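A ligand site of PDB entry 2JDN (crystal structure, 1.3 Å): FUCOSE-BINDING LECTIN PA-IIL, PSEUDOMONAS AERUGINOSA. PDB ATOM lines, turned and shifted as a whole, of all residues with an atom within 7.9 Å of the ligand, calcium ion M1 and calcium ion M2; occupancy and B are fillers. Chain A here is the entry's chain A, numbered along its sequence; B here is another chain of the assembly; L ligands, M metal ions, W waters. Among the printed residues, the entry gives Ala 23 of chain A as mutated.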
ATOM      1  N   ALA A  21     -11.083 -21.194 -23.608  1.00  0.00           N
ATOM      2  CA  ALA A  21     -10.230 -21.420 -24.793  1.00  0.00           C
ATOM      3  C   ALA A  21      -9.123 -22.412 -24.483  1.00  0.00           C
ATOM      4  O   ALA A  21      -8.533 -22.383 -23.408  1.00  0.00           O
ATOM      5  CB  ALA A  21      -9.664 -20.099 -25.288  1.00  0.00           C
ATOM      6  N   ASN A  22      -8.846 -23.259 -25.486  1.00  0.00           N
ATOM      7  CA  ASN A  22      -7.774 -24.263 -25.413  1.00  0.00           C
ATOM      8  C   ASN A  22      -7.176 -24.459 -26.796  1.00  0.00           C
ATOM      9  O   ASN A  22      -7.425 -25.462 -27.457  1.00  0.00           O
ATOM     10  CB  ASN A  22      -8.295 -25.613 -24.919  1.00  0.00           C
ATOM     11  CG  ASN A  22      -8.700 -25.579 -23.464  1.00  0.00           C
ATOM     12  OD1 ASN A  22      -7.832 -25.609 -22.587  1.00  0.00           O
ATOM     13  ND2 ASN A  22     -10.013 -25.502 -23.191  1.00  0.00           N
ATOM     14  N   ALA A  23      -6.420 -23.468 -27.275  1.00  0.00           N
ATOM     15  CA  ALA A  23      -5.939 -23.494 -28.654  1.00  0.00           C
ATOM     16  C   ALA A  23      -4.915 -22.406 -28.873  1.00  0.00           C
ATOM     17  O   ALA A  23      -4.915 -21.389 -28.168  1.00  0.00           O
ATOM     18  CB  ALA A  23      -7.123 -23.272 -29.633  1.00  0.00           C
ATOM     19  N   SER A  24      -4.063 -22.585 -29.893  1.00  0.00           N
ATOM     20  CA  SER A  24      -3.100 -21.544 -30.259  1.00  0.00           C
ATOM     21  C   SER A  24      -3.779 -20.263 -30.759  1.00  0.00           C
ATOM     22  O   SER A  24      -3.279 -19.173 -30.510  1.00  0.00           O
ATOM     23  CB  SER A  24      -2.133 -22.067 -31.331  1.00  0.00           C
ATOM     24  OG  SER A  24      -2.795 -22.272 -32.578  1.00  0.00           O
ATOM     25  N   GLY A  25      -4.901 -20.414 -31.477  1.00  0.00           N
ATOM     26  CA  GLY A  25      -5.508 -19.256 -32.119  1.00  0.00           C
ATOM     27  C   GLY A  25      -6.570 -18.564 -31.289  1.00  0.00           C
ATOM     28  O   GLY A  25      -7.207 -19.200 -30.410  1.00  0.00           O
ATOM     29  N   GLN A  27     -10.010 -17.360 -30.289  1.00  0.00           N
ATOM     30  CA  GLN A  27     -11.378 -17.844 -30.495  1.00  0.00           C
ATOM     31  C   GLN A  27     -12.346 -16.689 -30.407  1.00  0.00           C
ATOM     32  O   GLN A  27     -12.266 -15.896 -29.450  1.00  0.00           O
ATOM     33  CB  GLN A  27     -11.744 -18.862 -29.392  1.00  0.00           C
ATOM     34  CG  GLN A  27     -10.697 -19.941 -29.160  1.00  0.00           C
ATOM     35  CD  GLN A  27     -10.680 -20.957 -30.275  1.00  0.00           C
ATOM     36  OE1 GLN A  27     -11.713 -21.545 -30.631  1.00  0.00           O
ATOM     37  NE2 GLN A  27      -9.506 -21.170 -30.849  1.00  0.00           N
ATOM     38  N   GLN A  44      -7.629 -15.771 -26.255  1.00  0.00           N
ATOM     39  CA  GLN A  44      -6.724 -16.835 -26.600  1.00  0.00           C
ATOM     40  C   GLN A  44      -6.147 -17.440 -25.337  1.00  0.00           C
ATOM     41  O   GLN A  44      -5.710 -16.695 -24.435  1.00  0.00           O
ATOM     42  CB  GLN A  44      -5.597 -16.280 -27.507  1.00  0.00           C
ATOM     43  CG  GLN A  44      -4.651 -17.363 -28.088  1.00  0.00           C
ATOM     44  CD  GLN A  44      -3.601 -17.850 -27.091  1.00  0.00           C
ATOM     45  OE1 GLN A  44      -3.011 -17.026 -26.370  1.00  0.00           O
ATOM     46  NE2 GLN A  44      -3.355 -19.155 -27.034  1.00  0.00           N
ATOM     47  N   SER A  45      -6.129 -18.759 -25.273  1.00  0.00           N
ATOM     48  CA  SER A  45      -5.530 -19.471 -24.148  1.00  0.00           C
ATOM     49  C   SER A  45      -5.298 -20.897 -24.557  1.00  0.00           C
ATOM     50  O   SER A  45      -6.108 -21.466 -25.300  1.00  0.00           O
ATOM     51  CB  SER A  45      -6.491 -19.448 -22.936  1.00  0.00           C
ATOM     52  OG  SER A  45      -5.942 -20.198 -21.850  1.00  0.00           O
ATOM     53  N   THR A  46      -4.224 -21.516 -24.063  1.00  0.00           N
ATOM     54  CA  THR A  46      -4.058 -22.958 -24.148  1.00  0.00           C
ATOM     55  C   THR A  46      -4.230 -23.606 -22.767  1.00  0.00           C
ATOM     56  O   THR A  46      -3.888 -24.767 -22.591  1.00  0.00           O
ATOM     57  CB  THR A  46      -2.696 -23.360 -24.760  1.00  0.00           C
ATOM     58  OG1 THR A  46      -1.672 -22.615 -24.100  1.00  0.00           O
ATOM     59  CG2 THR A  46      -2.688 -23.065 -26.241  1.00  0.00           C
ATOM     60  N   VAL A  70     -12.456 -19.002 -35.780  1.00  0.00           N
ATOM     61  CA  VAL A  70     -11.011 -18.927 -35.483  1.00  0.00           C
ATOM     62  C   VAL A  70     -10.279 -18.724 -36.803  1.00  0.00           C
ATOM     63  O   VAL A  70     -10.564 -19.445 -37.775  1.00  0.00           O
ATOM     64  CB  VAL A  70     -10.481 -20.229 -34.846  1.00  0.00           C
ATOM     65  CG1 VAL A  70      -9.023 -20.101 -34.443  1.00  0.00           C
ATOM     66  CG2 VAL A  70     -11.318 -20.602 -33.640  1.00  0.00           C
ATOM     67  N   SER A  95     -15.812 -27.305 -29.785  1.00  0.00           N
ATOM     68  CA  SER A  95     -15.543 -26.829 -31.132  1.00  0.00           C
ATOM     69  C   SER A  95     -14.125 -27.176 -31.526  1.00  0.00           C
ATOM     70  O   SER A  95     -13.210 -27.220 -30.689  1.00  0.00           O
ATOM     71  CB  SER A  95     -15.787 -25.332 -31.279  1.00  0.00           C
ATOM     72  OG  SER A  95     -14.894 -24.567 -30.476  1.00  0.00           O
ATOM     73  N   GLU A  96     -13.937 -27.432 -32.833  1.00  0.00           N
ATOM     74  CA  GLU A  96     -12.650 -27.811 -33.394  1.00  0.00           C
ATOM     75  C   GLU A  96     -12.270 -26.836 -34.507  1.00  0.00           C
ATOM     76  O   GLU A  96     -13.005 -26.672 -35.493  1.00  0.00           O
ATOM     77  CB  GLU A  96     -12.697 -29.242 -33.913  1.00  0.00           C
ATOM     78  CG  GLU A  96     -11.398 -29.716 -34.564  1.00  0.00           C
ATOM     79  CD  GLU A  96     -10.211 -29.561 -33.644  1.00  0.00           C
ATOM     80  OE1 GLU A  96     -10.290 -30.014 -32.474  1.00  0.00           O
ATOM     81  OE2 GLU A  96      -9.177 -28.974 -34.044  1.00  0.00           O
ATOM     82  N   ASP A  97     -11.114 -26.204 -34.319  1.00  0.00           N
ATOM     83  CA  ASP A  97     -10.608 -25.212 -35.262  1.00  0.00           C
ATOM     84  C   ASP A  97      -9.524 -25.731 -36.174  1.00  0.00           C
ATOM     85  O   ASP A  97      -9.052 -24.970 -37.042  1.00  0.00           O
ATOM     86  CB  ASP A  97     -10.097 -23.961 -34.502  1.00  0.00           C
ATOM     87  CG  ASP A  97      -8.867 -24.205 -33.685  1.00  0.00           C
ATOM     88  OD1 ASP A  97      -8.097 -25.143 -33.970  1.00  0.00           O
ATOM     89  OD2 ASP A  97      -8.633 -23.388 -32.761  1.00  0.00           O
ATOM     90  N   GLY A  98      -9.139 -26.998 -36.023  1.00  0.00           N
ATOM     91  CA  GLY A  98      -7.938 -27.513 -36.685  1.00  0.00           C
ATOM     92  C   GLY A  98      -8.104 -28.961 -37.080  1.00  0.00           C
ATOM     93  O   GLY A  98      -9.149 -29.363 -37.619  1.00  0.00           O
ATOM     94  N   THR A  99      -7.084 -29.739 -36.759  1.00  0.00           N
ATOM     95  CA  THR A  99      -6.944 -31.082 -37.313  1.00  0.00           C
ATOM     96  C   THR A  99      -6.856 -32.157 -36.241  1.00  0.00           C
ATOM     97  O   THR A  99      -6.985 -33.345 -36.548  1.00  0.00           O
ATOM     98  CB  THR A  99      -5.697 -31.174 -38.207  1.00  0.00           C
ATOM     99  OG1 THR A  99      -4.566 -30.806 -37.432  1.00  0.00           O
ATOM    100  CG2 THR A  99      -5.811 -30.246 -39.418  1.00  0.00           C
ATOM    101  N   ASP A 100      -6.638 -31.789 -34.982  1.00  0.00           N
ATOM    102  CA  ASP A 100      -6.398 -32.804 -33.952  1.00  0.00           C
ATOM    103  C   ASP A 100      -7.674 -33.390 -33.326  1.00  0.00           C
ATOM    104  O   ASP A 100      -7.588 -34.364 -32.597  1.00  0.00           O
ATOM    105  CB  ASP A 100      -5.439 -32.322 -32.843  1.00  0.00           C
ATOM    106  CG  ASP A 100      -6.031 -31.226 -31.961  1.00  0.00           C
ATOM    107  OD1 ASP A 100      -7.084 -30.642 -32.331  1.00  0.00           O
ATOM    108  OD2 ASP A 100      -5.403 -30.918 -30.936  1.00  0.00           O
ATOM    109  N   ASN A 101      -8.818 -32.789 -33.624  1.00  0.00           N
ATOM    110  CA  ASN A 101     -10.119 -33.291 -33.146  1.00  0.00           C
ATOM    111  C   ASN A 101     -10.213 -33.457 -31.632  1.00  0.00           C
ATOM    112  O   ASN A 101     -10.891 -34.365 -31.145  1.00  0.00           O
ATOM    113  CB  ASN A 101     -10.500 -34.551 -33.911  1.00  0.00           C
ATOM    114  CG  ASN A 101     -10.706 -34.272 -35.375  1.00  0.00           C
ATOM    115  OD1 ASN A 101     -11.025 -33.148 -35.786  1.00  0.00           O
ATOM    116  ND2 ASN A 101     -10.537 -35.305 -36.184  1.00  0.00           N
ATOM    117  N   ASP A 102      -9.603 -32.538 -30.889  1.00  0.00           N
ATOM    118  CA  ASP A 102      -9.838 -32.520 -29.447  1.00  0.00           C
ATOM    119  C   ASP A 102     -11.154 -31.783 -29.098  1.00  0.00           C
ATOM    120  O   ASP A 102     -11.711 -32.025 -28.027  1.00  0.00           O
ATOM    121  CB  ASP A 102      -8.619 -32.012 -28.633  1.00  0.00           C
ATOM    122  CG  ASP A 102      -8.238 -30.528 -28.906  1.00  0.00           C
ATOM    123  OD1 ASP A 102      -8.829 -29.885 -29.792  1.00  0.00           O
ATOM    124  OD2 ASP A 102      -7.310 -30.043 -28.189  1.00  0.00           O
ATOM    125  N   TYR A 103     -11.685 -30.982 -30.004  1.00  0.00           N
ATOM    126  CA  TYR A 103     -12.972 -30.315 -29.815  1.00  0.00           C
ATOM    127  C   TYR A 103     -13.075 -29.427 -28.564  1.00  0.00           C
ATOM    128  O   TYR A 103     -14.182 -29.135 -28.098  1.00  0.00           O
ATOM    129  CB  TYR A 103     -14.157 -31.321 -29.927  1.00  0.00           C
ATOM    130  CG  TYR A 103     -14.467 -31.574 -31.395  1.00  0.00           C
ATOM    131  CD1 TYR A 103     -15.387 -30.786 -32.062  1.00  0.00           C
ATOM    132  CD2 TYR A 103     -13.754 -32.527 -32.121  1.00  0.00           C
ATOM    133  CE1 TYR A 103     -15.643 -30.986 -33.402  1.00  0.00           C
ATOM    134  CE2 TYR A 103     -13.978 -32.705 -33.461  1.00  0.00           C
ATOM    135  CZ  TYR A 103     -14.900 -31.932 -34.088  1.00  0.00           C
ATOM    136  OH  TYR A 103     -15.104 -32.115 -35.458  1.00  0.00           O
ATOM    137  N   ASN A 104     -11.935 -28.954 -28.052  1.00  0.00           N
ATOM    138  CA  ASN A 104     -11.931 -28.129 -26.846  1.00  0.00           C
ATOM    139  C   ASN A 104     -11.437 -26.719 -27.136  1.00  0.00           C
ATOM    140  O   ASN A 104     -11.184 -25.956 -26.232  1.00  0.00           O
ATOM    141  CB  ASN A 104     -11.064 -28.771 -25.765  1.00  0.00           C
ATOM    142  CG  ASN A 104      -9.583 -28.664 -26.072  1.00  0.00           C
ATOM    143  OD1 ASN A 104      -9.223 -28.132 -27.138  1.00  0.00           O
ATOM    144  ND2 ASN A 104      -8.733 -29.104 -25.173  1.00  0.00           N
ATOM    145  N   ASP A 105     -11.324 -26.378 -28.411  1.00  0.00           N
ATOM    146  CA  ASP A 105     -10.591 -25.157 -28.782  1.00  0.00           C
ATOM    147  C   ASP A 105     -11.325 -23.930 -28.258  1.00  0.00           C
ATOM    148  O   ASP A 105     -10.699 -23.014 -27.710  1.00  0.00           O
ATOM    149  CB  ASP A 105     -10.366 -25.133 -30.292  1.00  0.00           C
ATOM    150  CG  ASP A 105      -9.550 -26.308 -30.769  1.00  0.00           C
ATOM    151  OD1 ASP A 105      -8.623 -26.772 -30.036  1.00  0.00           O
ATOM    152  OD2 ASP A 105      -9.831 -26.823 -31.871  1.00  0.00           O
ATOM    153  N   ALA A 106     -12.652 -23.921 -28.409  1.00  0.00           N
ATOM    154  CA  ALA A 106     -13.529 -23.114 -27.554  1.00  0.00           C
ATOM    155  C   ALA A 106     -14.551 -24.056 -26.989  1.00  0.00           C
ATOM    156  O   ALA A 106     -15.161 -24.842 -27.742  1.00  0.00           O
ATOM    157  CB  ALA A 106     -14.231 -22.003 -28.315  1.00  0.00           C
ATOM    158  N   PRO B 113     -10.166 -33.002 -22.097  1.00  0.00           N
ATOM    159  CA  PRO B 113      -8.816 -32.481 -21.886  1.00  0.00           C
ATOM    160  C   PRO B 113      -8.741 -31.009 -22.181  1.00  0.00           C
ATOM    161  O   PRO B 113      -9.630 -30.401 -22.802  1.00  0.00           O
ATOM    162  CB  PRO B 113      -7.967 -33.295 -22.898  1.00  0.00           C
ATOM    163  CG  PRO B 113      -8.889 -33.525 -24.002  1.00  0.00           C
ATOM    164  CD  PRO B 113     -10.270 -33.757 -23.367  1.00  0.00           C
ATOM    165  N   LEU B 114      -7.626 -30.443 -21.735  1.00  0.00           N
ATOM    166  CA  LEU B 114      -7.276 -29.042 -21.982  1.00  0.00           C
ATOM    167  C   LEU B 114      -6.190 -28.956 -23.053  1.00  0.00           C
ATOM    168  O   LEU B 114      -5.721 -29.968 -23.564  1.00  0.00           O
ATOM    169  CB  LEU B 114      -6.786 -28.402 -20.682  1.00  0.00           C
ATOM    170  CG  LEU B 114      -7.735 -28.489 -19.482  1.00  0.00           C
ATOM    171  CD1 LEU B 114      -7.147 -27.674 -18.333  1.00  0.00           C
ATOM    172  CD2 LEU B 114      -9.168 -28.062 -19.843  1.00  0.00           C
ATOM    173  N   GLY B 115      -5.827 -27.745 -23.414  1.00  0.00           N
ATOM    174  CA  GLY B 115      -4.686 -27.500 -24.313  1.00  0.00           C
ATOM    175  C   GLY B 115      -5.019 -27.452 -25.770  1.00  0.00           C
ATOM    176  O   GLY B 115      -6.075 -27.957 -26.237  1.00  0.00           O
ATOM    177  OXT GLY B 115      -4.178 -26.918 -26.516  1.00  0.00           O
HETATM  178  C1  LIG L   1      -4.744 -25.617 -32.219  1.00  0.00           C
HETATM  179  C2  LIG L   1      -5.836 -26.553 -31.695  1.00  0.00           C
HETATM  180  C3  LIG L   1      -5.207 -27.755 -31.012  1.00  0.00           C
HETATM  181  C4  LIG L   1      -4.266 -27.301 -29.924  1.00  0.00           C
HETATM  182  C5  LIG L   1      -3.258 -26.281 -30.452  1.00  0.00           C
HETATM  183  C6  LIG L   1      -2.366 -25.686 -29.362  1.00  0.00           C
HETATM  184  O1  LIG L   1      -4.034 -26.303 -33.246  1.00  0.00           O
HETATM  185  O2  LIG L   1      -6.706 -27.024 -32.726  1.00  0.00           O
HETATM  186  O3  LIG L   1      -6.313 -28.521 -30.479  1.00  0.00           O
HETATM  187  O4  LIG L   1      -5.058 -26.725 -28.888  1.00  0.00           O
HETATM  188  O5  LIG L   1      -3.897 -25.215 -31.151  1.00  0.00           O
HETATM  189 CA    CA M   1      -7.255 -27.661 -28.336  1.00  0.00          CA
HETATM  190 CA    CA M   2      -8.323 -28.716 -31.786  1.00  0.00          CA
HETATM  191  O   HOH W   1      -5.418 -28.859 -34.624  1.00  0.00           O
HETATM  192  O   HOH W   2      -4.181 -26.379 -36.507  1.00  0.00           O
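OD1 of Asp 97 sits close to O2 of the ligand, at 2.6 Å. N of Ser 24 lies within hydrogen-bond range of O5 of the ligand, at 2.9 Å. OG of Ser 24 sits at hydrogen-bond distance from O5 of the ligand, 3.5 Å away.
The side-chain amide nitrogen (ND2) of Asn 104 lies within hydrogen-bond range of the backbone carbonyl oxygen (O) of Pro 113 of chain B, at 2.8 Å. The backbone NH of Asp 97 sits close to the side-chain carboxylate of Asp 105 (2.8 Å). The backbone NH of Asp 105 is in hydrogen-bond range of the backbone carbonyl oxygen of Ser 95 (3.1 Å). O of Ser 45 lies close to N of Asn 22. The side-chain carboxylate (OE1) of Glu 96 sits close to the backbone NH (N) of Tyr 103. N of Asn 101 lies close to OE1 of Glu 96 (3.3 Å). NE2 of Gln 44 sits close to O of Ser 24. The backbone NH (N) of Ala 23 lies within hydrogen-bond range of the backbone carbonyl oxygen (O) of Ser 45, 2.8 Å away.
Residues that only touch the ligand: Ala 23 (3.4 Å). Of the 25 residues printed, 9 come within 4 Å of the ligand. The nearest printed residue that does not touch the ligand is Thr 46 (4.1 Å).
Five residues have an atom within 4 Å of calcium ion M1: Asn 22, Asp 102, Asn 104, Asp 105 and Gly 115 of chain B. The nearest printed residue that does not touch calcium ion M1 is Ala 23 (4.4 Å).
The nearest printed residue that does not touch calcium ion M2 is Asp 97 (4.2 Å).
Calcium ion M1 is bound by the side-chain amide oxygen (OD1) of Asn 104, the side-chain carboxylate (OD1) of Asp 105, the backbone carbonyl oxygen (O) of Asn 22, the side-chain carboxylate (OD2) of Asp 102, the chain-end carboxylate (O) of Gly 115 of chain B, an oxygen (O4) of the ligand and an oxygen (O3) of the ligand. Slightly farther from calcium ion M1 lies the side-chain carboxylate (OD1) of Asp 102 (3.1 Å).
Calcium ion M2 is bound by OD1 of Asp 100 (2.4 Å), OD1 of Asp 102 (2.4 Å), O3 of the ligand (2.4 Å), OD2 of Asp 105 (2.4 Å), OE2 of Glu 96 (2.4 Å), OE1 of Glu 96 (2.5 Å), O2 of the ligand (2.5 Å) and OD1 of Asp 105 (2.6 Å). Calcium ion M2 has eight donor atoms within binding distance.
Water W1 lies within hydrogen-bond range of N of Thr 99 (2.8 Å), N of Asp 100 (3.2 Å) and O1 of the ligand (3.2 Å).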
